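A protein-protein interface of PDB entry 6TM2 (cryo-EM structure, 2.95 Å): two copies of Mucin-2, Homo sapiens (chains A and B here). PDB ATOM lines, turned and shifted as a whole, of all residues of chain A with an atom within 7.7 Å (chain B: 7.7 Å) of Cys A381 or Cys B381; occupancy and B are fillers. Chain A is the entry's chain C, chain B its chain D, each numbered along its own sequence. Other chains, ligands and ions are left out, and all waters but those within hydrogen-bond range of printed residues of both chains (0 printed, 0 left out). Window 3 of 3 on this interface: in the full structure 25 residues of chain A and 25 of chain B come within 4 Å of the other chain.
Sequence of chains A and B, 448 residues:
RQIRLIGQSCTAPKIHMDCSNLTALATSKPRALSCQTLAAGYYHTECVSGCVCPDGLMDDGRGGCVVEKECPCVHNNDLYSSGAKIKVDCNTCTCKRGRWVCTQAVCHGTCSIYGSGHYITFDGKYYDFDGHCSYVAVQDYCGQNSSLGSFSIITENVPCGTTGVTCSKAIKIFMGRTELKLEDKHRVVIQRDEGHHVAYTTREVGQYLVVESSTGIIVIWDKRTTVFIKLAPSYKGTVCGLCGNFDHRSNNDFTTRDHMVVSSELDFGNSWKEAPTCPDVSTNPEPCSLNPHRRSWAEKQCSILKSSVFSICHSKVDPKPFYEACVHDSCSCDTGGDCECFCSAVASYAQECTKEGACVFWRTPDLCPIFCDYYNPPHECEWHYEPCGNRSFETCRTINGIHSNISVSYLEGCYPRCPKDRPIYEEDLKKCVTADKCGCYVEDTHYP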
ATOM      1  N   CYS A 372      -0.263  27.957  15.303  1.00  0.00           N
ATOM      2  CA  CYS A 372      -1.254  28.713  14.553  1.00  0.00           C
ATOM      3  C   CYS A 372      -1.784  27.985  13.338  1.00  0.00           C
ATOM      4  O   CYS A 372      -2.809  28.397  12.799  1.00  0.00           O
ATOM      5  CB  CYS A 372      -0.695  30.064  14.087  1.00  0.00           C
ATOM      6  SG  CYS A 372      -0.365  31.304  15.352  1.00  0.00           S
ATOM      7  N   ASP A 373      -1.118  26.939  12.879  1.00  0.00           N
ATOM      8  CA  ASP A 373      -1.670  26.132  11.810  1.00  0.00           C
ATOM      9  C   ASP A 373      -2.589  25.042  12.328  1.00  0.00           C
ATOM     10  O   ASP A 373      -3.019  24.192  11.550  1.00  0.00           O
ATOM     11  CB  ASP A 373      -0.554  25.560  10.921  1.00  0.00           C
ATOM     12  CG  ASP A 373       0.496  24.781  11.688  1.00  0.00           C
ATOM     13  OD1 ASP A 373       0.462  24.773  12.930  1.00  0.00           O
ATOM     14  OD2 ASP A 373       1.362  24.163  11.034  1.00  0.00           O
ATOM     15  N   ASN A 376      -6.111  25.975  10.679  1.00  0.00           N
ATOM     16  CA  ASN A 376      -6.304  26.019   9.244  1.00  0.00           C
ATOM     17  C   ASN A 376      -7.329  24.974   8.822  1.00  0.00           C
ATOM     18  O   ASN A 376      -7.414  23.911   9.440  1.00  0.00           O
ATOM     19  CB  ASN A 376      -4.999  25.763   8.505  1.00  0.00           C
ATOM     20  CG  ASN A 376      -4.025  26.893   8.627  1.00  0.00           C
ATOM     21  OD1 ASN A 376      -4.403  28.053   8.658  1.00  0.00           O
ATOM     22  ND2 ASN A 376      -2.752  26.567   8.606  1.00  0.00           N
ATOM     23  N   PRO A 377      -8.138  25.266   7.809  1.00  0.00           N
ATOM     24  CA  PRO A 377      -8.806  24.201   7.074  1.00  0.00           C
ATOM     25  C   PRO A 377      -7.765  23.291   6.452  1.00  0.00           C
ATOM     26  O   PRO A 377      -6.800  23.798   5.863  1.00  0.00           O
ATOM     27  CB  PRO A 377      -9.617  24.959   6.015  1.00  0.00           C
ATOM     28  CG  PRO A 377      -8.927  26.262   5.866  1.00  0.00           C
ATOM     29  CD  PRO A 377      -8.393  26.591   7.217  1.00  0.00           C
ATOM     30  N   PRO A 378      -8.006  21.952   6.452  1.00  0.00           N
ATOM     31  CA  PRO A 378      -6.949  20.951   6.724  1.00  0.00           C
ATOM     32  C   PRO A 378      -5.529  21.219   6.245  1.00  0.00           C
ATOM     33  O   PRO A 378      -4.588  21.063   7.028  1.00  0.00           O
ATOM     34  CB  PRO A 378      -7.506  19.689   6.055  1.00  0.00           C
ATOM     35  CG  PRO A 378      -8.971  19.865   6.122  1.00  0.00           C
ATOM     36  CD  PRO A 378      -9.224  21.320   5.919  1.00  0.00           C
ATOM     37  N   HIS A 379      -5.350  21.642   4.988  1.00  0.00           N
ATOM     38  CA  HIS A 379      -4.021  22.054   4.547  1.00  0.00           C
ATOM     39  C   HIS A 379      -4.046  23.300   3.667  1.00  0.00           C
ATOM     40  O   HIS A 379      -3.076  23.550   2.941  1.00  0.00           O
ATOM     41  CB  HIS A 379      -3.305  20.913   3.827  1.00  0.00           C
ATOM     42  CG  HIS A 379      -2.950  19.776   4.732  1.00  0.00           C
ATOM     43  ND1 HIS A 379      -3.807  18.725   4.973  1.00  0.00           N
ATOM     44  CD2 HIS A 379      -1.857  19.556   5.498  1.00  0.00           C
ATOM     45  CE1 HIS A 379      -3.243  17.890   5.827  1.00  0.00           C
ATOM     46  NE2 HIS A 379      -2.059  18.371   6.162  1.00  0.00           N
ATOM     47  N   GLU A 380      -5.120  24.083   3.714  1.00  0.00           N
ATOM     48  CA  GLU A 380      -5.144  25.425   3.146  1.00  0.00           C
ATOM     49  C   GLU A 380      -4.708  26.394   4.231  1.00  0.00           C
ATOM     50  O   GLU A 380      -5.327  26.456   5.295  1.00  0.00           O
ATOM     51  CB  GLU A 380      -6.528  25.792   2.619  1.00  0.00           C
ATOM     52  CG  GLU A 380      -6.608  27.197   2.031  1.00  0.00           C
ATOM     53  CD  GLU A 380      -5.784  27.376   0.766  1.00  0.00           C
ATOM     54  OE1 GLU A 380      -5.576  26.388   0.031  1.00  0.00           O
ATOM     55  OE2 GLU A 380      -5.337  28.513   0.509  1.00  0.00           O
ATOM     56  N   CYS A 381      -3.668  27.158   3.953  1.00  0.00           N
ATOM     57  CA  CYS A 381      -2.869  27.802   4.986  1.00  0.00           C
ATOM     58  C   CYS A 381      -3.229  29.279   5.032  1.00  0.00           C
ATOM     59  O   CYS A 381      -2.696  30.078   4.261  1.00  0.00           O
ATOM     60  CB  CYS A 381      -1.394  27.583   4.681  1.00  0.00           C
ATOM     61  SG  CYS A 381      -0.199  28.061   5.923  1.00  0.00           S
ATOM     62  N   GLU A 382      -4.131  29.646   5.944  1.00  0.00           N
ATOM     63  CA  GLU A 382      -4.553  31.031   6.090  1.00  0.00           C
ATOM     64  C   GLU A 382      -4.194  31.660   7.428  1.00  0.00           C
ATOM     65  O   GLU A 382      -3.901  32.851   7.460  1.00  0.00           O
ATOM     66  CB  GLU A 382      -6.066  31.158   5.846  1.00  0.00           C
ATOM     67  CG  GLU A 382      -6.963  30.492   6.860  1.00  0.00           C
ATOM     68  CD  GLU A 382      -8.426  30.577   6.489  1.00  0.00           C
ATOM     69  OE1 GLU A 382      -8.730  31.085   5.396  1.00  0.00           O
ATOM     70  OE2 GLU A 382      -9.277  30.160   7.298  1.00  0.00           O
ATOM     71  N   TRP A 383      -4.174  30.901   8.521  1.00  0.00           N
ATOM     72  CA  TRP A 383      -3.858  31.445   9.838  1.00  0.00           C
ATOM     73  C   TRP A 383      -2.348  31.508   9.999  1.00  0.00           C
ATOM     74  O   TRP A 383      -1.680  30.475  10.058  1.00  0.00           O
ATOM     75  CB  TRP A 383      -4.492  30.593  10.932  1.00  0.00           C
ATOM     76  CG  TRP A 383      -5.969  30.740  11.061  1.00  0.00           C
ATOM     77  CD1 TRP A 383      -6.916  30.022  10.409  1.00  0.00           C
ATOM     78  CD2 TRP A 383      -6.672  31.579  11.974  1.00  0.00           C
ATOM     79  NE1 TRP A 383      -8.165  30.403  10.807  1.00  0.00           N
ATOM     80  CE2 TRP A 383      -8.043  31.356  11.777  1.00  0.00           C
ATOM     81  CE3 TRP A 383      -6.279  32.514  12.923  1.00  0.00           C
ATOM     82  CZ2 TRP A 383      -9.014  32.035  12.489  1.00  0.00           C
ATOM     83  CZ3 TRP A 383      -7.243  33.181  13.631  1.00  0.00           C
ATOM     84  CH2 TRP A 383      -8.594  32.943  13.410  1.00  0.00           C
ATOM     85  N   HIS A 384      -1.810  32.717  10.084  1.00  0.00           N
ATOM     86  CA  HIS A 384      -0.386  32.931  10.248  1.00  0.00           C
ATOM     87  C   HIS A 384      -0.124  33.570  11.599  1.00  0.00           C
ATOM     88  O   HIS A 384      -0.969  34.290  12.129  1.00  0.00           O
ATOM     89  CB  HIS A 384       0.168  33.835   9.147  1.00  0.00           C
ATOM     90  CG  HIS A 384       0.036  33.268   7.770  1.00  0.00           C
ATOM     91  ND1 HIS A 384      -1.063  33.505   6.975  1.00  0.00           N
ATOM     92  CD2 HIS A 384       0.846  32.452   7.057  1.00  0.00           C
ATOM     93  CE1 HIS A 384      -0.916  32.877   5.824  1.00  0.00           C
ATOM     94  NE2 HIS A 384       0.232  32.226   5.851  1.00  0.00           N
ATOM     95  N   ARG A 417      -5.764  35.400   7.034  1.00  0.00           N
ATOM     96  CA  ARG A 417      -5.393  36.059   5.793  1.00  0.00           C
ATOM     97  C   ARG A 417      -6.294  35.514   4.677  1.00  0.00           C
ATOM     98  O   ARG A 417      -5.837  34.883   3.731  1.00  0.00           O
ATOM     99  CB  ARG A 417      -3.899  35.898   5.517  1.00  0.00           C
ATOM    100  CG  ARG A 417      -3.389  36.789   4.406  1.00  0.00           C
ATOM    101  CD  ARG A 417      -1.897  36.736   4.260  1.00  0.00           C
ATOM    102  NE  ARG A 417      -1.224  37.325   5.407  1.00  0.00           N
ATOM    103  CZ  ARG A 417       0.091  37.310   5.572  1.00  0.00           C
ATOM    104  NH1 ARG A 417       0.861  36.759   4.651  1.00  0.00           N
ATOM    105  NH2 ARG A 417       0.638  37.866   6.640  1.00  0.00           N
ATOM    106  N   CYS A 418      -7.620  35.654   4.867  1.00  0.00           N
ATOM    107  CA  CYS A 418      -8.739  35.163   4.051  1.00  0.00           C
ATOM    108  C   CYS A 418      -8.531  35.282   2.540  1.00  0.00           C
ATOM    109  O   CYS A 418      -7.970  36.278   2.069  1.00  0.00           O
ATOM    110  CB  CYS A 418     -10.018  35.919   4.429  1.00  0.00           C
ATOM    111  SG  CYS A 418     -10.631  35.672   6.102  1.00  0.00           S
ATOM    112  N   CYS B 372       5.594  24.779  13.514  1.00  0.00           N
ATOM    113  CA  CYS B 372       6.109  24.281  12.247  1.00  0.00           C
ATOM    114  C   CYS B 372       6.089  25.307  11.136  1.00  0.00           C
ATOM    115  O   CYS B 372       6.747  25.094  10.120  1.00  0.00           O
ATOM    116  CB  CYS B 372       5.326  23.051  11.770  1.00  0.00           C
ATOM    117  SG  CYS B 372       5.517  21.530  12.714  1.00  0.00           S
ATOM    118  N   ASP B 373       5.350  26.393  11.282  1.00  0.00           N
ATOM    119  CA  ASP B 373       5.418  27.462  10.306  1.00  0.00           C
ATOM    120  C   ASP B 373       6.531  28.446  10.610  1.00  0.00           C
ATOM    121  O   ASP B 373       6.622  29.480   9.951  1.00  0.00           O
ATOM    122  CB  ASP B 373       4.059  28.166  10.165  1.00  0.00           C
ATOM    123  CG  ASP B 373       3.500  28.678  11.477  1.00  0.00           C
ATOM    124  OD1 ASP B 373       4.078  28.392  12.539  1.00  0.00           O
ATOM    125  OD2 ASP B 373       2.470  29.385  11.440  1.00  0.00           O
ATOM    126  N   ASN B 376       8.907  28.133   7.408  1.00  0.00           N
ATOM    127  CA  ASN B 376       8.446  28.444   6.071  1.00  0.00           C
ATOM    128  C   ASN B 376       9.237  29.616   5.504  1.00  0.00           C
ATOM    129  O   ASN B 376       9.645  30.504   6.255  1.00  0.00           O
ATOM    130  CB  ASN B 376       6.965  28.795   6.067  1.00  0.00           C
ATOM    131  CG  ASN B 376       6.083  27.615   6.333  1.00  0.00           C
ATOM    132  OD1 ASN B 376       6.370  26.505   5.916  1.00  0.00           O
ATOM    133  ND2 ASN B 376       4.952  27.865   6.953  1.00  0.00           N
ATOM    134  N   PRO B 377       9.500  29.621   4.201  1.00  0.00           N
ATOM    135  CA  PRO B 377       9.835  30.866   3.524  1.00  0.00           C
ATOM    136  C   PRO B 377       8.679  31.838   3.662  1.00  0.00           C
ATOM    137  O   PRO B 377       7.527  31.433   3.456  1.00  0.00           O
ATOM    138  CB  PRO B 377      10.053  30.429   2.070  1.00  0.00           C
ATOM    139  CG  PRO B 377       9.294  29.162   1.934  1.00  0.00           C
ATOM    140  CD  PRO B 377       9.393  28.491   3.260  1.00  0.00           C
ATOM    141  N   PRO B 378       8.970  33.149   3.876  1.00  0.00           N
ATOM    142  CA  PRO B 378       8.199  33.995   4.815  1.00  0.00           C
ATOM    143  C   PRO B 378       6.700  33.770   4.963  1.00  0.00           C
ATOM    144  O   PRO B 378       6.212  33.681   6.091  1.00  0.00           O
ATOM    145  CB  PRO B 378       8.474  35.410   4.291  1.00  0.00           C
ATOM    146  CG  PRO B 378       9.806  35.306   3.663  1.00  0.00           C
ATOM    147  CD  PRO B 378       9.863  33.957   3.029  1.00  0.00           C
ATOM    148  N   HIS B 379       5.964  33.649   3.853  1.00  0.00           N
ATOM    149  CA  HIS B 379       4.556  33.280   3.957  1.00  0.00           C
ATOM    150  C   HIS B 379       4.119  32.284   2.888  1.00  0.00           C
ATOM    151  O   HIS B 379       2.917  32.160   2.627  1.00  0.00           O
ATOM    152  CB  HIS B 379       3.660  34.518   3.922  1.00  0.00           C
ATOM    153  CG  HIS B 379       3.805  35.384   5.133  1.00  0.00           C
ATOM    154  ND1 HIS B 379       4.738  36.394   5.216  1.00  0.00           N
ATOM    155  CD2 HIS B 379       3.176  35.353   6.330  1.00  0.00           C
ATOM    156  CE1 HIS B 379       4.656  36.968   6.402  1.00  0.00           C
ATOM    157  NE2 HIS B 379       3.716  36.356   7.097  1.00  0.00           N
ATOM    158  N   GLU B 380       5.058  31.574   2.268  1.00  0.00           N
ATOM    159  CA  GLU B 380       4.754  30.410   1.447  1.00  0.00           C
ATOM    160  C   GLU B 380       4.787  29.187   2.346  1.00  0.00           C
ATOM    161  O   GLU B 380       5.807  28.908   2.979  1.00  0.00           O
ATOM    162  CB  GLU B 380       5.742  30.258   0.293  1.00  0.00           C
ATOM    163  CG  GLU B 380       5.474  29.040  -0.586  1.00  0.00           C
ATOM    164  CD  GLU B 380       4.169  29.122  -1.361  1.00  0.00           C
ATOM    165  OE1 GLU B 380       3.715  30.244  -1.670  1.00  0.00           O
ATOM    166  OE2 GLU B 380       3.591  28.055  -1.658  1.00  0.00           O
ATOM    167  N   CYS B 381       3.690  28.453   2.381  1.00  0.00           N
ATOM    168  CA  CYS B 381       3.393  27.538   3.474  1.00  0.00           C
ATOM    169  C   CYS B 381       3.652  26.115   3.003  1.00  0.00           C
ATOM    170  O   CYS B 381       2.790  25.495   2.380  1.00  0.00           O
ATOM    171  CB  CYS B 381       1.949  27.740   3.912  1.00  0.00           C
ATOM    172  SG  CYS B 381       1.399  26.913   5.399  1.00  0.00           S
ATOM    173  N   GLU B 382       4.841  25.593   3.308  1.00  0.00           N
ATOM    174  CA  GLU B 382       5.206  24.239   2.917  1.00  0.00           C
ATOM    175  C   GLU B 382       5.438  23.289   4.083  1.00  0.00           C
ATOM    176  O   GLU B 382       5.124  22.111   3.955  1.00  0.00           O
ATOM    177  CB  GLU B 382       6.446  24.260   2.009  1.00  0.00           C
ATOM    178  CG  GLU B 382       7.735  24.713   2.651  1.00  0.00           C
ATOM    179  CD  GLU B 382       8.877  24.802   1.664  1.00  0.00           C
ATOM    180  OE1 GLU B 382       8.639  24.588   0.464  1.00  0.00           O
ATOM    181  OE2 GLU B 382      10.019  25.061   2.089  1.00  0.00           O
ATOM    182  N   TRP B 383       5.944  23.764   5.218  1.00  0.00           N
ATOM    183  CA  TRP B 383       6.210  22.904   6.368  1.00  0.00           C
ATOM    184  C   TRP B 383       4.925  22.720   7.157  1.00  0.00           C
ATOM    185  O   TRP B 383       4.411  23.670   7.749  1.00  0.00           O
ATOM    186  CB  TRP B 383       7.308  23.505   7.238  1.00  0.00           C
ATOM    187  CG  TRP B 383       8.680  23.415   6.665  1.00  0.00           C
ATOM    188  CD1 TRP B 383       9.282  24.320   5.855  1.00  0.00           C
ATOM    189  CD2 TRP B 383       9.666  22.423   6.945  1.00  0.00           C
ATOM    190  NE1 TRP B 383      10.555  23.926   5.557  1.00  0.00           N
ATOM    191  CE2 TRP B 383      10.819  22.764   6.225  1.00  0.00           C
ATOM    192  CE3 TRP B 383       9.679  21.270   7.718  1.00  0.00           C
ATOM    193  CZ2 TRP B 383      11.965  21.991   6.251  1.00  0.00           C
ATOM    194  CZ3 TRP B 383      10.817  20.507   7.746  1.00  0.00           C
ATOM    195  CH2 TRP B 383      11.943  20.867   7.017  1.00  0.00           C
ATOM    196  N   HIS B 384       4.413  21.497   7.180  1.00  0.00           N
ATOM    197  CA  HIS B 384       3.197  21.171   7.898  1.00  0.00           C
ATOM    198  C   HIS B 384       3.522  20.214   9.030  1.00  0.00           C
ATOM    199  O   HIS B 384       4.471  19.437   8.945  1.00  0.00           O
ATOM    200  CB  HIS B 384       2.164  20.525   6.974  1.00  0.00           C
ATOM    201  CG  HIS B 384       1.709  21.411   5.859  1.00  0.00           C
ATOM    202  ND1 HIS B 384       2.329  21.433   4.630  1.00  0.00           N
ATOM    203  CD2 HIS B 384       0.714  22.326   5.793  1.00  0.00           C
ATOM    204  CE1 HIS B 384       1.726  22.308   3.849  1.00  0.00           C
ATOM    205  NE2 HIS B 384       0.746  22.868   4.533  1.00  0.00           N
ATOM    206  N   ARG B 417       6.458  19.844   2.162  1.00  0.00           N
ATOM    207  CA  ARG B 417       5.542  19.479   1.094  1.00  0.00           C
ATOM    208  C   ARG B 417       5.892  20.323  -0.139  1.00  0.00           C
ATOM    209  O   ARG B 417       5.101  21.134  -0.609  1.00  0.00           O
ATOM    210  CB  ARG B 417       4.092  19.618   1.550  1.00  0.00           C
ATOM    211  CG  ARG B 417       3.096  18.989   0.600  1.00  0.00           C
ATOM    212  CD  ARG B 417       1.697  18.994   1.143  1.00  0.00           C
ATOM    213  NE  ARG B 417       1.564  18.112   2.291  1.00  0.00           N
ATOM    214  CZ  ARG B 417       0.460  18.014   3.017  1.00  0.00           C
ATOM    215  NH1 ARG B 417      -0.604  18.724   2.689  1.00  0.00           N
ATOM    216  NH2 ARG B 417       0.408  17.189   4.050  1.00  0.00           N
ATOM    217  N   CYS B 418       7.157  20.216  -0.588  1.00  0.00           N
ATOM    218  CA  CYS B 418       7.829  20.953  -1.667  1.00  0.00           C
ATOM    219  C   CYS B 418       6.976  21.189  -2.915  1.00  0.00           C
ATOM    220  O   CYS B 418       6.208  20.308  -3.319  1.00  0.00           O
ATOM    221  CB  CYS B 418       9.100  20.208  -2.084  1.00  0.00           C
ATOM    222  SG  CYS B 418      10.402  20.084  -0.849  1.00  0.00           S
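The backbone carbonyl oxygen (O) of Glu B382 is in hydrogen-bond range of the backbone NH (N) of Arg B417 (3.2 Å).
O of Glu B382 lies within hydrogen-bond range of ND1 of His B384 (3.0 Å).
ND1 of His A384 sits at hydrogen-bond distance from O of Glu A382 (3.0 Å).
The backbone carbonyl oxygen (O) of Glu A382 lies within hydrogen-bond range of the backbone NH (N) of Arg A417 (3.2 Å).
Among the printed residues, pairs that only touch across the chains: His A379 with His B384 (3.8 Å) and His A384 with His B379 (3.8 Å).
Of the printed residues of chain B, Cys A381 touches Cys B381.
Of the printed residues of chain A, Cys B381 touches Cys A381 (2.0 Å).
Of the printed residues of chain B, Arg A417 touches His B379.
Printed residues of chain A within 4 Å of His B379: His A384 (3.8 Å) and Arg A417 (3.2 Å).
The nearest printed residue of chain A that does not touch His B384 is Asp A373 (4.7 Å).
NE2 of His A379 is in hydrogen-bond range of NH2 of Arg B417.
A ring nitrogen (NE2) of His B379 lies within hydrogen-bond range of the guanidinium group of Arg A417 (3.5 Å).
SG of Cys A381 forms a disulfide with SG of Cys B381, at 2.0 Å.
Hydrophobic or aromatic side chains of chain B that line the printed part of chain A: His B379 and His B384.
Of the 13 printed residues of chain A, 4 touch a printed residue of chain B.
Hydrophobic or aromatic side chains of chain A within 4 Å of the printed part of chain B: His A379 and His A384.
Among the printed residues, 5 pairs touch across the chains.
His A379 touches His B384, and with the chains exchanged His A384 touches His B379.
His A379 touches Arg B417, and with the chains exchanged Arg A417 touches His B379.
Cys A381 touches its own counterpart, Cys B381.
Positions printed for both chains: 372, 373, 376, 377, 378, 379, 380, 381, 382, 383, 384, 417 and 418.
Of the 5 pairs that touch across the chains among the printed residues, 5 have their exchanged pair printed and touching as well.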
